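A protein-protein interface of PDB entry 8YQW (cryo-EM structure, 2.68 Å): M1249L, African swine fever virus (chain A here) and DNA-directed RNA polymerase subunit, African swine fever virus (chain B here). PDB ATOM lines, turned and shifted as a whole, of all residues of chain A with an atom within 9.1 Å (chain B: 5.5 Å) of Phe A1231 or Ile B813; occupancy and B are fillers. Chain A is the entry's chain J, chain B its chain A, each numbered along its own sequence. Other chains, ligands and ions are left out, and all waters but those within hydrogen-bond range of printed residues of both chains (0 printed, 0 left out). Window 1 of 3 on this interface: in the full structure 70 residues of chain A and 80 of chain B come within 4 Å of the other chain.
Of the printed residues of chain B, Phe A1231 touches Ile B813, Ala B816, Leu B817 and Ser B820. Printed residues of chain A within 4 Å of Ser B820: Pro A1230 (2.3 Å), Phe A1231 (3.6 Å) and Ser A1232 (3.2 Å). Of the printed residues of chain B, Pro A1230 touches Leu B817 (3.3 Å) and Ser B820 (2.3 Å). Printed residues of chain B within 4 Å of Leu A1246: Lys B815 (3.4 Å). Ile A1233 touches none of the printed residues of chain B. The nearest printed residue of chain B that does not touch Phe A1231 is Leu B812 (5.8 Å). The nearest printed residue of chain A that does not touch Ala B816 is Pro A1230 (5.3 Å).
The backbone carbonyl oxygen (O) of Asp A1229 is in hydrogen-bond range of the side-chain hydroxyl (OG) of Ser A1232, 3.3 Å away. The backbone NH of Phe A1231 lies close to the side-chain carboxylate of Asp A1229 (3.3 Å). O of Leu B817 sits at hydrogen-bond distance from OG of Ser B820 (3.5 Å). O of Lys B815 lies within hydrogen-bond range of OG of Ser B818 (3.0 Å).
Of the 11 printed residues of chain A, 5 touch a printed residue of chain B. Printed residues of chain B that touch a printed residue of chain A: Ile B813, Lys B815, Ala B816, Leu B817 and Ser B820. Hydrophobic or aromatic side chains of chain B within 4 Å of the printed part of chain A: Ile B813, Ala B816 and Leu B817. Among the printed residues, 9 pairs touch across the chains. Among the printed residues, no Asp or Glu carboxylate lies within 4 Å of a Lys or Arg side-chain nitrogen of the other chain.
The side-chain hydroxyl (OG) of Ser B820 sits close to the backbone carbonyl oxygen (O) of Pro A1230. The side-chain amino group (NZ) of Lys B815 lies within hydrogen-bond range of the backbone carbonyl oxygen (O) of Leu A1246 (3.4 Å).
Pro A1230 touches Leu B817. CZ of Phe A1231 touches CG2 of Ile B813 (3.6 Å). Phe A1231 touches Ala B816 (CE2 to CB, 3.99 Å). CG of Leu B817 touches CZ of Phe A1231 (3.5 Å). Phe A1231 touches Ser B820 (CA to OG, 3.6 Å). Ser B820 touches Ser A1232. Pro A1248 touches Lys B815 (CB to CG, 3.8 Å).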
ATOM      1  N   ASP A1228      29.424  16.310 -13.455  1.00  0.00           N
ATOM      2  CA  ASP A1228      28.741  15.747 -12.301  1.00  0.00           C
ATOM      3  C   ASP A1228      29.150  14.294 -12.110  1.00  0.00           C
ATOM      4  O   ASP A1228      29.360  13.563 -13.080  1.00  0.00           O
ATOM      5  CB  ASP A1228      27.223  15.838 -12.473  1.00  0.00           C
ATOM      6  CG  ASP A1228      26.636  17.085 -11.843  1.00  0.00           C
ATOM      7  OD1 ASP A1228      27.162  17.535 -10.804  1.00  0.00           O
ATOM      8  OD2 ASP A1228      25.644  17.615 -12.387  1.00  0.00           O
ATOM      9  N   ASP A1229      29.265  13.883 -10.854  1.00  0.00           N
ATOM     10  CA  ASP A1229      29.535  12.485 -10.546  1.00  0.00           C
ATOM     11  C   ASP A1229      28.262  11.678 -10.762  1.00  0.00           C
ATOM     12  O   ASP A1229      27.261  11.929 -10.082  1.00  0.00           O
ATOM     13  CB  ASP A1229      30.021  12.343  -9.110  1.00  0.00           C
ATOM     14  CG  ASP A1229      30.690  11.008  -8.843  1.00  0.00           C
ATOM     15  OD1 ASP A1229      30.454  10.044  -9.598  1.00  0.00           O
ATOM     16  OD2 ASP A1229      31.460  10.927  -7.864  1.00  0.00           O
ATOM     17  N   PRO A1230      28.248  10.716 -11.688  1.00  0.00           N
ATOM     18  CA  PRO A1230      27.007   9.975 -11.957  1.00  0.00           C
ATOM     19  C   PRO A1230      26.524   9.133 -10.790  1.00  0.00           C
ATOM     20  O   PRO A1230      25.340   8.779 -10.760  1.00  0.00           O
ATOM     21  CB  PRO A1230      27.373   9.100 -13.162  1.00  0.00           C
ATOM     22  CG  PRO A1230      28.857   9.013 -13.136  1.00  0.00           C
ATOM     23  CD  PRO A1230      29.336  10.319 -12.596  1.00  0.00           C
ATOM     24  N   PHE A1231      27.388   8.804  -9.833  1.00  0.00           N
ATOM     25  CA  PHE A1231      27.023   7.934  -8.724  1.00  0.00           C
ATOM     26  C   PHE A1231      26.830   8.678  -7.412  1.00  0.00           C
ATOM     27  O   PHE A1231      26.432   8.060  -6.422  1.00  0.00           O
ATOM     28  CB  PHE A1231      28.081   6.844  -8.540  1.00  0.00           C
ATOM     29  CG  PHE A1231      27.955   5.708  -9.510  1.00  0.00           C
ATOM     30  CD1 PHE A1231      28.507   5.795 -10.776  1.00  0.00           C
ATOM     31  CD2 PHE A1231      27.285   4.553  -9.157  1.00  0.00           C
ATOM     32  CE1 PHE A1231      28.393   4.753 -11.666  1.00  0.00           C
ATOM     33  CE2 PHE A1231      27.169   3.507 -10.044  1.00  0.00           C
ATOM     34  CZ  PHE A1231      27.724   3.607 -11.300  1.00  0.00           C
ATOM     35  N   SER A1232      27.094   9.980  -7.377  1.00  0.00           N
ATOM     36  CA  SER A1232      26.982  10.754  -6.149  1.00  0.00           C
ATOM     37  C   SER A1232      25.537  11.179  -5.933  1.00  0.00           C
ATOM     38  O   SER A1232      24.876  11.652  -6.861  1.00  0.00           O
ATOM     39  CB  SER A1232      27.888  11.984  -6.198  1.00  0.00           C
ATOM     40  OG  SER A1232      27.322  13.002  -7.004  1.00  0.00           O
ATOM     41  N   ILE A1233      25.054  11.010  -4.707  1.00  0.00           N
ATOM     42  CA  ILE A1233      23.701  11.459  -4.346  1.00  0.00           C
ATOM     43  C   ILE A1233      23.852  12.898  -3.863  1.00  0.00           C
ATOM     44  O   ILE A1233      23.924  13.197  -2.670  1.00  0.00           O
ATOM     45  CB  ILE A1233      23.042  10.541  -3.312  1.00  0.00           C
ATOM     46  CG1 ILE A1233      24.017  10.202  -2.184  1.00  0.00           C
ATOM     47  CG2 ILE A1233      22.558   9.263  -3.975  1.00  0.00           C
ATOM     48  CD1 ILE A1233      23.349   9.649  -0.954  1.00  0.00           C
ATOM     49  N   GLU A1234      23.896  13.817  -4.824  1.00  0.00           N
ATOM     50  CA  GLU A1234      24.030  15.239  -4.537  1.00  0.00           C
ATOM     51  C   GLU A1234      22.705  15.980  -4.612  1.00  0.00           C
ATOM     52  O   GLU A1234      22.464  16.890  -3.814  1.00  0.00           O
ATOM     53  CB  GLU A1234      25.031  15.881  -5.502  1.00  0.00           C
ATOM     54  CG  GLU A1234      25.465  17.284  -5.111  1.00  0.00           C
ATOM     55  CD  GLU A1234      26.355  17.308  -3.881  1.00  0.00           C
ATOM     56  OE1 GLU A1234      26.862  16.237  -3.483  1.00  0.00           O
ATOM     57  OE2 GLU A1234      26.551  18.402  -3.312  1.00  0.00           O
ATOM     58  N   ASP A1235      21.841  15.617  -5.553  1.00  0.00           N
ATOM     59  CA  ASP A1235      20.508  16.194  -5.636  1.00  0.00           C
ATOM     60  C   ASP A1235      19.466  15.370  -4.895  1.00  0.00           C
ATOM     61  O   ASP A1235      18.286  15.733  -4.907  1.00  0.00           O
ATOM     62  CB  ASP A1235      20.094  16.365  -7.100  1.00  0.00           C
ATOM     63  CG  ASP A1235      20.826  17.503  -7.785  1.00  0.00           C
ATOM     64  OD1 ASP A1235      21.616  18.196  -7.112  1.00  0.00           O
ATOM     65  OD2 ASP A1235      20.596  17.720  -8.991  1.00  0.00           O
ATOM     66  N   VAL A1236      19.868  14.281  -4.253  1.00  0.00           N
ATOM     67  CA  VAL A1236      18.969  13.451  -3.462  1.00  0.00           C
ATOM     68  C   VAL A1236      19.142  13.852  -2.005  1.00  0.00           C
ATOM     69  O   VAL A1236      20.212  13.656  -1.419  1.00  0.00           O
ATOM     70  CB  VAL A1236      19.248  11.957  -3.666  1.00  0.00           C
ATOM     71  CG1 VAL A1236      18.234  11.121  -2.903  1.00  0.00           C
ATOM     72  CG2 VAL A1236      19.228  11.614  -5.142  1.00  0.00           C
ATOM     73  N   LEU A1246      18.002   2.532   0.160  1.00  0.00           N
ATOM     74  CA  LEU A1246      18.447   2.425  -1.221  1.00  0.00           C
ATOM     75  C   LEU A1246      19.017   1.055  -1.552  1.00  0.00           C
ATOM     76  O   LEU A1246      19.478   0.850  -2.679  1.00  0.00           O
ATOM     77  CB  LEU A1246      19.493   3.503  -1.516  1.00  0.00           C
ATOM     78  CG  LEU A1246      19.089   4.937  -1.174  1.00  0.00           C
ATOM     79  CD1 LEU A1246      20.204   5.908  -1.505  1.00  0.00           C
ATOM     80  CD2 LEU A1246      17.812   5.318  -1.898  1.00  0.00           C
ATOM     81  N   PRO A1248      19.460  -2.580  -2.886  1.00  0.00           N
ATOM     82  CA  PRO A1248      18.748  -3.208  -4.011  1.00  0.00           C
ATOM     83  C   PRO A1248      17.741  -4.252  -3.576  1.00  0.00           C
ATOM     84  O   PRO A1248      16.756  -4.478  -4.291  1.00  0.00           O
ATOM     85  CB  PRO A1248      19.880  -3.825  -4.839  1.00  0.00           C
ATOM     86  CG  PRO A1248      20.981  -4.030  -3.875  1.00  0.00           C
ATOM     87  CD  PRO A1248      20.893  -2.912  -2.884  1.00  0.00           C
ATOM     88  N   ARG B 809      26.266  -7.945 -12.096  1.00  0.00           N
ATOM     89  CA  ARG B 809      26.918  -6.720 -11.655  1.00  0.00           C
ATOM     90  C   ARG B 809      26.227  -5.486 -12.221  1.00  0.00           C
ATOM     91  O   ARG B 809      26.181  -4.445 -11.558  1.00  0.00           O
ATOM     92  CB  ARG B 809      28.395  -6.747 -12.049  1.00  0.00           C
ATOM     93  CG  ARG B 809      29.183  -5.517 -11.650  1.00  0.00           C
ATOM     94  CD  ARG B 809      29.197  -5.320 -10.149  1.00  0.00           C
ATOM     95  NE  ARG B 809      29.760  -6.467  -9.450  1.00  0.00           N
ATOM     96  CZ  ARG B 809      31.046  -6.617  -9.173  1.00  0.00           C
ATOM     97  NH1 ARG B 809      31.941  -5.714  -9.533  1.00  0.00           N
ATOM     98  NH2 ARG B 809      31.446  -7.703  -8.520  1.00  0.00           N
ATOM     99  N   PHE B 810      25.680  -5.587 -13.434  1.00  0.00           N
ATOM    100  CA  PHE B 810      24.951  -4.465 -14.016  1.00  0.00           C
ATOM    101  C   PHE B 810      23.712  -4.124 -13.201  1.00  0.00           C
ATOM    102  O   PHE B 810      23.372  -2.948 -13.038  1.00  0.00           O
ATOM    103  CB  PHE B 810      24.565  -4.782 -15.457  1.00  0.00           C
ATOM    104  CG  PHE B 810      25.671  -4.563 -16.434  1.00  0.00           C
ATOM    105  CD1 PHE B 810      25.892  -3.313 -16.976  1.00  0.00           C
ATOM    106  CD2 PHE B 810      26.495  -5.603 -16.805  1.00  0.00           C
ATOM    107  CE1 PHE B 810      26.908  -3.109 -17.871  1.00  0.00           C
ATOM    108  CE2 PHE B 810      27.518  -5.404 -17.698  1.00  0.00           C
ATOM    109  CZ  PHE B 810      27.724  -4.157 -18.234  1.00  0.00           C
ATOM    110  N   ASP B 811      23.015  -5.140 -12.693  1.00  0.00           N
ATOM    111  CA  ASP B 811      21.838  -4.888 -11.869  1.00  0.00           C
ATOM    112  C   ASP B 811      22.195  -4.073 -10.633  1.00  0.00           C
ATOM    113  O   ASP B 811      21.406  -3.237 -10.182  1.00  0.00           O
ATOM    114  CB  ASP B 811      21.188  -6.213 -11.470  1.00  0.00           C
ATOM    115  CG  ASP B 811      20.803  -7.057 -12.669  1.00  0.00           C
ATOM    116  OD1 ASP B 811      20.587  -6.485 -13.756  1.00  0.00           O
ATOM    117  OD2 ASP B 811      20.711  -8.295 -12.523  1.00  0.00           O
ATOM    118  N   LEU B 812      23.379  -4.309 -10.065  1.00  0.00           N
ATOM    119  CA  LEU B 812      23.811  -3.535  -8.907  1.00  0.00           C
ATOM    120  C   LEU B 812      24.277  -2.143  -9.313  1.00  0.00           C
ATOM    121  O   LEU B 812      24.052  -1.171  -8.586  1.00  0.00           O
ATOM    122  CB  LEU B 812      24.923  -4.276  -8.170  1.00  0.00           C
ATOM    123  CG  LEU B 812      24.620  -5.728  -7.812  1.00  0.00           C
ATOM    124  CD1 LEU B 812      25.782  -6.337  -7.067  1.00  0.00           C
ATOM    125  CD2 LEU B 812      23.352  -5.815  -6.992  1.00  0.00           C
ATOM    126  N   ILE B 813      24.941  -2.030 -10.463  1.00  0.00           N
ATOM    127  CA  ILE B 813      25.406  -0.728 -10.930  1.00  0.00           C
ATOM    128  C   ILE B 813      24.227   0.146 -11.334  1.00  0.00           C
ATOM    129  O   ILE B 813      24.164   1.328 -10.978  1.00  0.00           O
ATOM    130  CB  ILE B 813      26.404  -0.904 -12.087  1.00  0.00           C
ATOM    131  CG1 ILE B 813      27.693  -1.552 -11.588  1.00  0.00           C
ATOM    132  CG2 ILE B 813      26.708   0.429 -12.737  1.00  0.00           C
ATOM    133  CD1 ILE B 813      28.581  -2.052 -12.697  1.00  0.00           C
ATOM    134  N   ASN B 814      23.272  -0.418 -12.075  1.00  0.00           N
ATOM    135  CA  ASN B 814      22.121   0.363 -12.513  1.00  0.00           C
ATOM    136  C   ASN B 814      21.220   0.745 -11.349  1.00  0.00           C
ATOM    137  O   ASN B 814      20.545   1.776 -11.407  1.00  0.00           O
ATOM    138  CB  ASN B 814      21.329  -0.407 -13.565  1.00  0.00           C
ATOM    139  CG  ASN B 814      22.068  -0.528 -14.878  1.00  0.00           C
ATOM    140  OD1 ASN B 814      21.873  -1.481 -15.626  1.00  0.00           O
ATOM    141  ND2 ASN B 814      22.926   0.439 -15.163  1.00  0.00           N
ATOM    142  N   LYS B 815      21.180  -0.070 -10.294  1.00  0.00           N
ATOM    143  CA  LYS B 815      20.408   0.298  -9.113  1.00  0.00           C
ATOM    144  C   LYS B 815      21.029   1.490  -8.399  1.00  0.00           C
ATOM    145  O   LYS B 815      20.316   2.400  -7.961  1.00  0.00           O
ATOM    146  CB  LYS B 815      20.290  -0.892  -8.165  1.00  0.00           C
ATOM    147  CG  LYS B 815      19.559  -0.583  -6.872  1.00  0.00           C
ATOM    148  CD  LYS B 815      18.065  -0.426  -7.102  1.00  0.00           C
ATOM    149  CE  LYS B 815      17.334  -0.085  -5.814  1.00  0.00           C
ATOM    150  NZ  LYS B 815      17.490   1.346  -5.446  1.00  0.00           N
ATOM    151  N   ALA B 816      22.355   1.501  -8.266  1.00  0.00           N
ATOM    152  CA  ALA B 816      23.026   2.632  -7.638  1.00  0.00           C
ATOM    153  C   ALA B 816      22.939   3.881  -8.501  1.00  0.00           C
ATOM    154  O   ALA B 816      22.919   4.998  -7.972  1.00  0.00           O
ATOM    155  CB  ALA B 816      24.485   2.285  -7.355  1.00  0.00           C
ATOM    156  N   LEU B 817      22.897   3.716  -9.823  1.00  0.00           N
ATOM    157  CA  LEU B 817      22.731   4.853 -10.716  1.00  0.00           C
ATOM    158  C   LEU B 817      21.295   5.352 -10.748  1.00  0.00           C
ATOM    159  O   LEU B 817      21.065   6.549 -10.942  1.00  0.00           O
ATOM    160  CB  LEU B 817      23.184   4.482 -12.126  1.00  0.00           C
ATOM    161  CG  LEU B 817      24.649   4.730 -12.469  1.00  0.00           C
ATOM    162  CD1 LEU B 817      25.053   3.927 -13.689  1.00  0.00           C
ATOM    163  CD2 LEU B 817      24.892   6.205 -12.699  1.00  0.00           C
ATOM    164  N   SER B 818      20.321   4.463 -10.552  1.00  0.00           N
ATOM    165  CA  SER B 818      18.921   4.866 -10.593  1.00  0.00           C
ATOM    166  C   SER B 818      18.538   5.785  -9.446  1.00  0.00           C
ATOM    167  O   SER B 818      17.447   6.359  -9.476  1.00  0.00           O
ATOM    168  CB  SER B 818      18.015   3.636 -10.587  1.00  0.00           C
ATOM    169  OG  SER B 818      17.764   3.199  -9.265  1.00  0.00           O
ATOM    170  N   SER B 820      20.988   8.289  -8.085  1.00  0.00           N
ATOM    171  CA  SER B 820      21.633   9.563  -8.378  1.00  0.00           C
ATOM    172  C   SER B 820      21.149  10.159  -9.697  1.00  0.00           C
ATOM    173  O   SER B 820      20.892  11.363  -9.773  1.00  0.00           O
ATOM    174  CB  SER B 820      23.148   9.386  -8.395  1.00  0.00           C
ATOM    175  OG  SER B 820      23.535   8.437  -9.371  1.00  0.00           O
